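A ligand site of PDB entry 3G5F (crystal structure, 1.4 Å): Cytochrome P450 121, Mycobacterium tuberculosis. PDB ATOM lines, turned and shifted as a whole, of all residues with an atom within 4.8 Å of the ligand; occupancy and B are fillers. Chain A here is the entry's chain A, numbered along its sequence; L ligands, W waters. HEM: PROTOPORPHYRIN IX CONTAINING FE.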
ATOM      1  N   LEU A  55       7.098 -16.457 -17.882  1.00  0.00           N
ATOM      2  CA  LEU A  55       7.764 -15.446 -17.044  1.00  0.00           C
ATOM      3  C   LEU A  55       6.872 -14.235 -16.731  1.00  0.00           C
ATOM      4  O   LEU A  55       7.096 -13.558 -15.726  1.00  0.00           O
ATOM      5  CB  LEU A  55       9.083 -14.992 -17.655  1.00  0.00           C
ATOM      6  CG  LEU A  55      10.193 -16.040 -17.680  1.00  0.00           C
ATOM      7  CD1 LEU A  55      11.413 -15.476 -18.389  1.00  0.00           C
ATOM      8  CD2 LEU A  55      10.563 -16.523 -16.260  1.00  0.00           C
ATOM      9  N   MET A  62       7.794 -17.954  -8.465  1.00  0.00           N
ATOM     10  CA  MET A  62       9.133 -18.208  -7.932  1.00  0.00           C
ATOM     11  C   MET A  62       9.024 -18.590  -6.459  1.00  0.00           C
ATOM     12  O   MET A  62       9.625 -19.578  -6.006  1.00  0.00           O
ATOM     13  CB  MET A  62      10.079 -17.004  -8.091  1.00  0.00           C
ATOM     14  CG  MET A  62      11.425 -17.138  -7.256  1.00  0.00           C
ATOM     15  SD  MET A  62      12.701 -18.135  -7.989  1.00  0.00           S
ATOM     16  CE  MET A  62      13.400 -16.913  -9.085  1.00  0.00           C
ATOM     17  N   MET A  86      13.466 -10.964  -3.249  1.00  0.00           N
ATOM     18  CA  MET A  86      13.009  -9.695  -3.800  1.00  0.00           C
ATOM     19  C   MET A  86      11.658  -9.265  -3.250  1.00  0.00           C
ATOM     20  O   MET A  86      11.446  -8.085  -2.916  1.00  0.00           O
ATOM     21  CB  MET A  86      13.026  -9.722  -5.322  1.00  0.00           C
ATOM     22  CG  MET A  86      14.427  -9.442  -5.889  1.00  0.00           C
ATOM     23  SD  MET A  86      15.257  -7.857  -5.535  1.00  0.00           S
ATOM     24  CE  MET A  86      13.833  -6.772  -5.280  1.00  0.00           C
ATOM     25  N   ILE A 102      22.622  -0.244  -6.726  1.00  0.00           N
ATOM     26  CA  ILE A 102      23.343  -1.214  -7.568  1.00  0.00           C
ATOM     27  C   ILE A 102      23.347  -0.859  -9.062  1.00  0.00           C
ATOM     28  O   ILE A 102      23.605  -1.721  -9.924  1.00  0.00           O
ATOM     29  CB  ILE A 102      22.848  -2.660  -7.350  1.00  0.00           C
ATOM     30  CG1 ILE A 102      21.389  -2.798  -7.785  1.00  0.00           C
ATOM     31  CG2 ILE A 102      23.080  -3.083  -5.868  1.00  0.00           C
ATOM     32  CD1 ILE A 102      20.884  -4.231  -7.865  1.00  0.00           C
ATOM     33  N   HIS A 146      31.859  -5.748  -6.865  1.00  0.00           N
ATOM     34  CA  HIS A 146      30.807  -5.920  -5.884  1.00  0.00           C
ATOM     35  C   HIS A 146      31.200  -5.490  -4.486  1.00  0.00           C
ATOM     36  O   HIS A 146      30.342  -5.009  -3.730  1.00  0.00           O
ATOM     37  CB  HIS A 146      30.194  -7.323  -5.954  1.00  0.00           C
ATOM     38  CG  HIS A 146      29.311  -7.493  -7.157  1.00  0.00           C
ATOM     39  ND1 HIS A 146      29.820  -7.733  -8.414  1.00  0.00           N
ATOM     40  CD2 HIS A 146      27.975  -7.379  -7.302  1.00  0.00           C
ATOM     41  CE1 HIS A 146      28.821  -7.751  -9.291  1.00  0.00           C
ATOM     42  NE2 HIS A 146      27.693  -7.560  -8.635  1.00  0.00           N
ATOM     43  N   PHE A 230      22.996 -10.308  -2.692  1.00  0.00           N
ATOM     44  CA  PHE A 230      23.387  -9.432  -3.800  1.00  0.00           C
ATOM     45  C   PHE A 230      24.864  -9.600  -4.163  1.00  0.00           C
ATOM     46  O   PHE A 230      25.215  -9.625  -5.346  1.00  0.00           O
ATOM     47  CB  PHE A 230      22.978  -7.965  -3.536  1.00  0.00           C
ATOM     48  CG  PHE A 230      21.553  -7.693  -3.911  1.00  0.00           C
ATOM     49  CD1 PHE A 230      20.507  -8.342  -3.235  1.00  0.00           C
ATOM     50  CD2 PHE A 230      21.231  -6.882  -5.002  1.00  0.00           C
ATOM     51  CE1 PHE A 230      19.184  -8.139  -3.607  1.00  0.00           C
ATOM     52  CE2 PHE A 230      19.908  -6.688  -5.372  1.00  0.00           C
ATOM     53  CZ  PHE A 230      18.887  -7.308  -4.657  1.00  0.00           C
ATOM     54  N   ALA A 233      24.850 -13.280  -5.984  1.00  0.00           N
ATOM     55  CA  ALA A 233      24.191 -13.260  -7.285  1.00  0.00           C
ATOM     56  C   ALA A 233      24.960 -12.393  -8.274  1.00  0.00           C
ATOM     57  O   ALA A 233      25.180 -12.784  -9.436  1.00  0.00           O
ATOM     58  CB  ALA A 233      22.755 -12.779  -7.152  1.00  0.00           C
ATOM     59  N   GLY A 234      25.402 -11.217  -7.830  1.00  0.00           N
ATOM     60  CA  GLY A 234      26.069 -10.301  -8.761  1.00  0.00           C
ATOM     61  C   GLY A 234      27.438 -10.833  -9.153  1.00  0.00           C
ATOM     62  O   GLY A 234      27.780 -10.808 -10.339  1.00  0.00           O
ATOM     63  N   SER A 237      27.111 -13.994 -11.360  1.00  0.00           N
ATOM     64  CA  SER A 237      26.460 -13.786 -12.639  1.00  0.00           C
ATOM     65  C   SER A 237      27.349 -12.977 -13.576  1.00  0.00           C
ATOM     66  O   SER A 237      27.483 -13.324 -14.764  1.00  0.00           O
ATOM     67  CB  SER A 237      25.128 -13.077 -12.445  1.00  0.00           C
ATOM     68  OG  SER A 237      24.244 -13.866 -11.670  1.00  0.00           O
ATOM     69  N   THR A 238      27.968 -11.932 -13.034  1.00  0.00           N
ATOM     70  CA  THR A 238      28.852 -11.092 -13.861  1.00  0.00           C
ATOM     71  C   THR A 238      30.148 -11.829 -14.196  1.00  0.00           C
ATOM     72  O   THR A 238      30.643 -11.762 -15.340  1.00  0.00           O
ATOM     73  CB  THR A 238      29.174  -9.707 -13.211  1.00  0.00           C
ATOM     74  OG1 THR A 238      29.775  -9.888 -11.946  1.00  0.00           O
ATOM     75  CG2 THR A 238      27.918  -8.872 -13.058  1.00  0.00           C
ATOM     76  N   PHE A 241      29.185 -14.610 -16.735  1.00  0.00           N
ATOM     77  CA  PHE A 241      28.808 -14.074 -18.036  1.00  0.00           C
ATOM     78  C   PHE A 241      30.036 -13.513 -18.765  1.00  0.00           C
ATOM     79  O   PHE A 241      30.268 -13.835 -19.940  1.00  0.00           O
ATOM     80  CB  PHE A 241      27.730 -12.973 -17.955  1.00  0.00           C
ATOM     81  CG  PHE A 241      27.567 -12.260 -19.258  1.00  0.00           C
ATOM     82  CD1 PHE A 241      27.136 -12.971 -20.367  1.00  0.00           C
ATOM     83  CD2 PHE A 241      27.978 -10.935 -19.413  1.00  0.00           C
ATOM     84  CE1 PHE A 241      27.045 -12.351 -21.635  1.00  0.00           C
ATOM     85  CE2 PHE A 241      27.894 -10.321 -20.659  1.00  0.00           C
ATOM     86  CZ  PHE A 241      27.435 -11.033 -21.768  1.00  0.00           C
ATOM     87  N   LEU A 274      25.129 -11.226 -24.615  1.00  0.00           N
ATOM     88  CA  LEU A 274      24.070 -11.586 -23.656  1.00  0.00           C
ATOM     89  C   LEU A 274      23.046 -12.496 -24.292  1.00  0.00           C
ATOM     90  O   LEU A 274      22.689 -13.538 -23.734  1.00  0.00           O
ATOM     91  CB  LEU A 274      23.387 -10.325 -23.106  1.00  0.00           C
ATOM     92  CG  LEU A 274      24.179  -9.600 -22.020  1.00  0.00           C
ATOM     93  CD1 LEU A 274      23.696  -8.152 -21.850  1.00  0.00           C
ATOM     94  CD2 LEU A 274      24.115 -10.352 -20.676  1.00  0.00           C
ATOM     95  N   PHE A 280      23.522 -19.530 -17.798  1.00  0.00           N
ATOM     96  CA  PHE A 280      22.574 -20.205 -16.904  1.00  0.00           C
ATOM     97  C   PHE A 280      22.498 -21.687 -17.238  1.00  0.00           C
ATOM     98  O   PHE A 280      22.128 -22.062 -18.350  1.00  0.00           O
ATOM     99  CB  PHE A 280      21.188 -19.549 -16.925  1.00  0.00           C
ATOM    100  CG  PHE A 280      21.066 -18.409 -15.960  1.00  0.00           C
ATOM    101  CD1 PHE A 280      21.830 -17.270 -16.114  1.00  0.00           C
ATOM    102  CD2 PHE A 280      20.192 -18.489 -14.888  1.00  0.00           C
ATOM    103  CE1 PHE A 280      21.727 -16.202 -15.206  1.00  0.00           C
ATOM    104  CE2 PHE A 280      20.075 -17.421 -13.980  1.00  0.00           C
ATOM    105  CZ  PHE A 280      20.839 -16.302 -14.131  1.00  0.00           C
ATOM    106  N   LEU A 284      14.969 -21.460 -15.670  1.00  0.00           N
ATOM    107  CA  LEU A 284      14.483 -20.745 -14.480  1.00  0.00           C
ATOM    108  C   LEU A 284      13.259 -21.462 -13.930  1.00  0.00           C
ATOM    109  O   LEU A 284      12.311 -21.734 -14.648  1.00  0.00           O
ATOM    110  CB  LEU A 284      14.085 -19.309 -14.859  1.00  0.00           C
ATOM    111  CG  LEU A 284      15.182 -18.471 -15.510  1.00  0.00           C
ATOM    112  CD1 LEU A 284      14.599 -17.104 -15.797  1.00  0.00           C
ATOM    113  CD2 LEU A 284      16.448 -18.366 -14.638  1.00  0.00           C
ATOM    114  N   ARG A 286       9.792 -22.292 -11.835  1.00  0.00           N
ATOM    115  CA  ARG A 286       8.558 -21.688 -11.350  1.00  0.00           C
ATOM    116  C   ARG A 286       7.608 -22.826 -10.952  1.00  0.00           C
ATOM    117  O   ARG A 286       7.622 -23.881 -11.571  1.00  0.00           O
ATOM    118  CB  ARG A 286       7.882 -20.887 -12.455  1.00  0.00           C
ATOM    119  CG  ARG A 286       8.656 -19.659 -12.943  1.00  0.00           C
ATOM    120  CD  ARG A 286       8.780 -18.585 -11.874  1.00  0.00           C
ATOM    121  NE  ARG A 286       9.327 -17.325 -12.379  1.00  0.00           N
ATOM    122  CZ  ARG A 286      10.612 -16.989 -12.379  1.00  0.00           C
ATOM    123  NH1 ARG A 286      11.555 -17.819 -11.934  1.00  0.00           N
ATOM    124  NH2 ARG A 286      10.968 -15.794 -12.829  1.00  0.00           N
ATOM    125  N   LEU A 309      16.364 -20.403 -20.947  1.00  0.00           N
ATOM    126  CA  LEU A 309      16.707 -19.100 -21.519  1.00  0.00           C
ATOM    127  C   LEU A 309      17.268 -19.215 -22.935  1.00  0.00           C
ATOM    128  O   LEU A 309      16.901 -18.403 -23.805  1.00  0.00           O
ATOM    129  CB  LEU A 309      17.654 -18.333 -20.615  1.00  0.00           C
ATOM    130  CG  LEU A 309      17.073 -17.989 -19.229  1.00  0.00           C
ATOM    131  CD1 LEU A 309      18.058 -17.164 -18.442  1.00  0.00           C
ATOM    132  CD2 LEU A 309      15.716 -17.255 -19.321  1.00  0.00           C
ATOM    133  N   LEU A 336      16.070 -12.770 -23.274  1.00  0.00           N
ATOM    134  CA  LEU A 336      15.708 -13.094 -21.895  1.00  0.00           C
ATOM    135  C   LEU A 336      16.941 -13.312 -21.006  1.00  0.00           C
ATOM    136  O   LEU A 336      16.829 -13.979 -19.955  1.00  0.00           O
ATOM    137  CB  LEU A 336      14.789 -14.320 -21.854  1.00  0.00           C
ATOM    138  CG  LEU A 336      13.502 -14.238 -22.705  1.00  0.00           C
ATOM    139  CD1 LEU A 336      12.596 -15.397 -22.315  1.00  0.00           C
ATOM    140  CD2 LEU A 336      12.771 -12.893 -22.612  1.00  0.00           C
ATOM    141  N   ALA A 337      18.115 -12.787 -21.386  1.00  0.00           N
ATOM    142  CA  ALA A 337      19.322 -13.037 -20.550  1.00  0.00           C
ATOM    143  C   ALA A 337      19.174 -12.561 -19.112  1.00  0.00           C
ATOM    144  O   ALA A 337      19.822 -13.097 -18.218  1.00  0.00           O
ATOM    145  CB  ALA A 337      20.572 -12.412 -21.161  1.00  0.00           C
ATOM    146  N   PHE A 338      18.348 -11.529 -18.892  1.00  0.00           N
ATOM    147  CA  PHE A 338      18.102 -10.971 -17.547  1.00  0.00           C
ATOM    148  C   PHE A 338      16.721 -11.373 -17.027  1.00  0.00           C
ATOM    149  O   PHE A 338      16.227 -10.772 -16.068  1.00  0.00           O
ATOM    150  CB  PHE A 338      18.247  -9.444 -17.565  1.00  0.00           C
ATOM    151  CG  PHE A 338      19.651  -8.970 -17.817  1.00  0.00           C
ATOM    152  CD1 PHE A 338      20.672  -9.251 -16.911  1.00  0.00           C
ATOM    153  CD2 PHE A 338      19.939  -8.180 -18.935  1.00  0.00           C
ATOM    154  CE1 PHE A 338      21.977  -8.795 -17.134  1.00  0.00           C
ATOM    155  CE2 PHE A 338      21.236  -7.715 -19.167  1.00  0.00           C
ATOM    156  CZ  PHE A 338      22.250  -7.995 -18.255  1.00  0.00           C
ATOM    157  N   GLY A 339      16.096 -12.364 -17.658  1.00  0.00           N
ATOM    158  CA  GLY A 339      14.728 -12.739 -17.323  1.00  0.00           C
ATOM    159  C   GLY A 339      13.716 -11.773 -17.898  1.00  0.00           C
ATOM    160  O   GLY A 339      14.006 -11.033 -18.855  1.00  0.00           O
ATOM    161  N   GLN A 342       8.098 -10.117 -13.254  1.00  0.00           N
ATOM    162  CA  GLN A 342       8.225  -9.784 -11.850  1.00  0.00           C
ATOM    163  C   GLN A 342       9.652  -9.902 -11.317  1.00  0.00           C
ATOM    164  O   GLN A 342      10.069  -9.127 -10.459  1.00  0.00           O
ATOM    165  CB  GLN A 342       7.272 -10.670 -11.045  1.00  0.00           C
ATOM    166  CG  GLN A 342       7.306 -10.450  -9.530  1.00  0.00           C
ATOM    167  CD  GLN A 342       6.542  -9.207  -9.066  1.00  0.00           C
ATOM    168  OE1 GLN A 342       6.550  -8.885  -7.866  1.00  0.00           O
ATOM    169  NE2 GLN A 342       5.870  -8.543  -9.979  1.00  0.00           N
ATOM    170  N   HIS A 343      10.410 -10.870 -11.833  1.00  0.00           N
ATOM    171  CA  HIS A 343      11.715 -11.165 -11.301  1.00  0.00           C
ATOM    172  C   HIS A 343      12.883 -10.739 -12.195  1.00  0.00           C
ATOM    173  O   HIS A 343      14.010 -11.200 -12.028  1.00  0.00           O
ATOM    174  CB  HIS A 343      11.795 -12.646 -10.907  1.00  0.00           C
ATOM    175  CG  HIS A 343      10.822 -12.991  -9.825  1.00  0.00           C
ATOM    176  ND1 HIS A 343      10.978 -12.535  -8.529  1.00  0.00           N
ATOM    177  CD2 HIS A 343       9.641 -13.665  -9.850  1.00  0.00           C
ATOM    178  CE1 HIS A 343       9.950 -12.958  -7.795  1.00  0.00           C
ATOM    179  NE2 HIS A 343       9.130 -13.636  -8.574  1.00  0.00           N
ATOM    180  N   PHE A 344      12.592  -9.800 -13.108  1.00  0.00           N
ATOM    181  CA  PHE A 344      13.609  -9.267 -14.008  1.00  0.00           C
ATOM    182  C   PHE A 344      14.816  -8.806 -13.185  1.00  0.00           C
ATOM    183  O   PHE A 344      14.692  -8.177 -12.121  1.00  0.00           O
ATOM    184  CB  PHE A 344      13.029  -8.088 -14.799  1.00  0.00           C
ATOM    185  CG  PHE A 344      14.004  -7.497 -15.769  1.00  0.00           C
ATOM    186  CD1 PHE A 344      14.184  -8.079 -17.019  1.00  0.00           C
ATOM    187  CD2 PHE A 344      14.785  -6.403 -15.417  1.00  0.00           C
ATOM    188  CE1 PHE A 344      15.115  -7.548 -17.922  1.00  0.00           C
ATOM    189  CE2 PHE A 344      15.739  -5.873 -16.326  1.00  0.00           C
ATOM    190  CZ  PHE A 344      15.890  -6.473 -17.560  1.00  0.00           C
ATOM    191  N   CYS A 345      16.027  -9.135 -13.666  1.00  0.00           N
ATOM    192  CA  CYS A 345      17.257  -8.871 -12.920  1.00  0.00           C
ATOM    193  C   CYS A 345      17.387  -7.428 -12.476  1.00  0.00           C
ATOM    194  O   CYS A 345      17.407  -6.543 -13.336  1.00  0.00           O
ATOM    195  CB  CYS A 345      18.470  -9.215 -13.802  1.00  0.00           C
ATOM    196  SG  CYS A 345      20.036  -8.935 -12.957  1.00  0.00           S
ATOM    197  N   PRO A 346      17.556  -7.185 -11.175  1.00  0.00           N
ATOM    198  CA  PRO A 346      17.730  -5.792 -10.734  1.00  0.00           C
ATOM    199  C   PRO A 346      19.146  -5.267 -10.980  1.00  0.00           C
ATOM    200  O   PRO A 346      19.393  -4.058 -10.818  1.00  0.00           O
ATOM    201  CB  PRO A 346      17.433  -5.858  -9.236  1.00  0.00           C
ATOM    202  CG  PRO A 346      17.886  -7.277  -8.829  1.00  0.00           C
ATOM    203  CD  PRO A 346      17.527  -8.127 -10.031  1.00  0.00           C
ATOM    204  N   GLY A 347      20.065  -6.160 -11.345  1.00  0.00           N
ATOM    205  CA  GLY A 347      21.437  -5.744 -11.623  1.00  0.00           C
ATOM    206  C   GLY A 347      21.766  -5.614 -13.110  1.00  0.00           C
ATOM    207  O   GLY A 347      22.938  -5.529 -13.449  1.00  0.00           O
ATOM    208  N   LEU A 350      24.207  -2.813 -14.206  1.00  0.00           N
ATOM    209  CA  LEU A 350      25.533  -3.077 -13.672  1.00  0.00           C
ATOM    210  C   LEU A 350      26.220  -4.223 -14.417  1.00  0.00           C
ATOM    211  O   LEU A 350      27.425  -4.147 -14.703  1.00  0.00           O
ATOM    212  CB  LEU A 350      25.476  -3.361 -12.172  1.00  0.00           C
ATOM    213  CG  LEU A 350      26.780  -3.446 -11.392  1.00  0.00           C
ATOM    214  CD1 LEU A 350      27.496  -2.112 -11.377  1.00  0.00           C
ATOM    215  CD2 LEU A 350      26.534  -3.892  -9.970  1.00  0.00           C
ATOM    216  N   GLY A 351      25.457  -5.268 -14.727  1.00  0.00           N
ATOM    217  CA  GLY A 351      26.015  -6.429 -15.432  1.00  0.00           C
ATOM    218  C   GLY A 351      26.482  -6.033 -16.827  1.00  0.00           C
ATOM    219  O   GLY A 351      27.559  -6.431 -17.280  1.00  0.00           O
HETATM  220  CHA HEM L   1      17.660 -12.166 -11.192  1.00  0.00           C
HETATM  221  CHB HEM L   1      20.706 -12.846 -14.897  1.00  0.00           C
HETATM  222  CHC HEM L   1      23.793  -9.665 -12.867  1.00  0.00           C
HETATM  223  CHD HEM L   1      21.191  -9.776  -8.825  1.00  0.00           C
HETATM  224  C1A HEM L   1      18.179 -12.539 -12.402  1.00  0.00           C
HETATM  225  C2A HEM L   1      17.498 -13.346 -13.395  1.00  0.00           C
HETATM  226  C3A HEM L   1      18.351 -13.552 -14.413  1.00  0.00           C
HETATM  227  C4A HEM L   1      19.578 -12.872 -14.099  1.00  0.00           C
HETATM  228  CMA HEM L   1      18.078 -14.391 -15.670  1.00  0.00           C
HETATM  229  CAA HEM L   1      16.046 -13.866 -13.324  1.00  0.00           C
HETATM  230  CBA HEM L   1      15.908 -15.093 -12.433  1.00  0.00           C
HETATM  231  CGA HEM L   1      14.494 -15.617 -12.439  1.00  0.00           C
HETATM  232  O1A HEM L   1      13.571 -14.918 -12.931  1.00  0.00           O
HETATM  233  O2A HEM L   1      14.255 -16.747 -11.932  1.00  0.00           O
HETATM  234  C1B HEM L   1      21.812 -12.042 -14.663  1.00  0.00           C
HETATM  235  C2B HEM L   1      22.938 -11.863 -15.562  1.00  0.00           C
HETATM  236  C3B HEM L   1      23.795 -10.981 -15.001  1.00  0.00           C
HETATM  237  C4B HEM L   1      23.239 -10.597 -13.730  1.00  0.00           C
HETATM  238  CMB HEM L   1      23.090 -12.569 -16.927  1.00  0.00           C
HETATM  239  CAB HEM L   1      25.123 -10.433 -15.543  1.00  0.00           C
HETATM  240  CBB HEM L   1      25.351 -10.228 -16.841  1.00  0.00           C
HETATM  241  C1C HEM L   1      23.317  -9.354 -11.614  1.00  0.00           C
HETATM  242  C2C HEM L   1      23.911  -8.418 -10.679  1.00  0.00           C
HETATM  243  C3C HEM L   1      23.182  -8.461  -9.543  1.00  0.00           C
HETATM  244  C4C HEM L   1      22.122  -9.414  -9.761  1.00  0.00           C
HETATM  245  CMC HEM L   1      25.155  -7.527 -10.966  1.00  0.00           C
HETATM  246  CAC HEM L   1      23.333  -7.673  -8.216  1.00  0.00           C
HETATM  247  CBC HEM L   1      24.381  -6.892  -7.937  1.00  0.00           C
HETATM  248  C1D HEM L   1      20.026 -10.464  -9.084  1.00  0.00           C
HETATM  249  C2D HEM L   1      19.011 -10.705  -8.096  1.00  0.00           C
HETATM  250  C3D HEM L   1      17.921 -11.420  -8.822  1.00  0.00           C
HETATM  251  C4D HEM L   1      18.375 -11.589 -10.182  1.00  0.00           C
HETATM  252  CMD HEM L   1      19.048 -10.309  -6.621  1.00  0.00           C
HETATM  253  CAD HEM L   1      16.611 -11.926  -8.222  1.00  0.00           C
HETATM  254  CBD HEM L   1      15.474 -11.010  -8.671  1.00  0.00           C
HETATM  255  CGD HEM L   1      14.132 -11.505  -8.167  1.00  0.00           C
HETATM  256  O1D HEM L   1      13.160 -10.738  -8.350  1.00  0.00           O
HETATM  257  O2D HEM L   1      14.046 -12.613  -7.614  1.00  0.00           O
HETATM  258  NA  HEM L   1      19.441 -12.279 -12.849  1.00  0.00           N
HETATM  259  NB  HEM L   1      22.042 -11.270 -13.532  1.00  0.00           N
HETATM  260  NC  HEM L   1      22.222  -9.948 -11.016  1.00  0.00           N
HETATM  261  ND  HEM L   1      19.644 -11.012 -10.301  1.00  0.00           N
HETATM  262 FE   HEM L   1      20.755 -10.956 -12.006  1.00  0.00          FE
HETATM  263  O   HOH W   1      12.637 -13.145 -14.723  1.00  0.00           O
HETATM  264  O   HOH W   2      10.568  -9.165  -7.742  1.00  0.00           O
HETATM  265  O   HOH W   3      15.908 -18.106 -10.403  1.00  0.00           O
HETATM  266  O   HOH W   4      13.366 -13.223  -5.085  1.00  0.00           O
HETATM  267  O   HOH W   5      21.615 -13.031 -10.981  1.00  0.00           O
HETATM  268  O   HOH W   6      15.946 -14.804  -6.845  1.00  0.00           O
HETATM  269  O   HOH W   7      13.600  -8.370  -9.546  1.00  0.00           O
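CE of Met 62 touches O2A of the ligand, at 3.0 Å. CG of Met 86 touches O1D of the ligand, at 3.1 Å. His 146 touches the ligand (NE2 to CMC, 3.4 Å). CZ of Phe 230 touches CMD of the ligand, 3.6 Å away. Ala 233 touches the ligand. CA of Gly 234 touches C2C of the ligand, 3.4 Å away. CB of Ser 237 touches C4B of the ligand (3.4 Å). Thr 238 touches the ligand. CD2 of Phe 241 touches CBB of the ligand (3.7 Å). CE1 of Phe 280 touches CHB of the ligand (3.5 Å). Leu 284 touches the ligand (CD1 to CGA, 3.7 Å). CD1 of Leu 309 touches CMA of the ligand, 3.9 Å away. Ala 337 touches the ligand (O to CMA, 3.3 Å). Phe 338 touches the ligand (CE1 to C3B, 3.6 Å). Gly 339 touches the ligand (N to CMA, 3.5 Å). CD of Pro 346 touches C3D of the ligand (3.5 Å). Gly 347 touches the ligand. 20 residues have an atom within 4 Å of the ligand: Met 62, Met 86, His 146, Phe 230, Ala 233, Gly 234, Ser 237, Thr 238, Phe 241, Phe 280, Leu 284, Arg 286, Leu 309, Ala 337, Phe 338, Gly 339, His 343, Cys 345, Pro 346 and Gly 347. The nearest printed residue that does not touch the ligand is Leu 350 (4.01 Å).
Water W4 bridges an oxygen (O2D) of the ligand (2.7 Å) and the backbone NH (N) of Met 86 (2.9 Å). Water W7 bridges an oxygen (O1D) of the ligand (2.7 Å) and the backbone carbonyl oxygen (O) of Phe 344 (2.8 Å). Water W2 lies within hydrogen-bond range of O of Gln 342, O1D of the ligand and ND1 of His 343.
O of Ala 233 is in hydrogen-bond range of OG of Ser 237, 2.7 Å away. N of Cys 345 sits at hydrogen-bond distance from O of Phe 338, at 2.9 Å. N of Gly 347 lies close to SG of Cys 345 (3.2 Å). OG1 of Thr 238 sits at hydrogen-bond distance from O of Gly 234 (2.7 Å).
FE of the ligand is bound by SG of Cys 345 (2.3 Å). The guanidinium group (NH2) of Arg 286 lies within salt-bridge range of an oxygen (O1A) of the ligand. ND1 of His 343 sits at hydrogen-bond distance from O1D of the ligand, at 2.8 Å.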
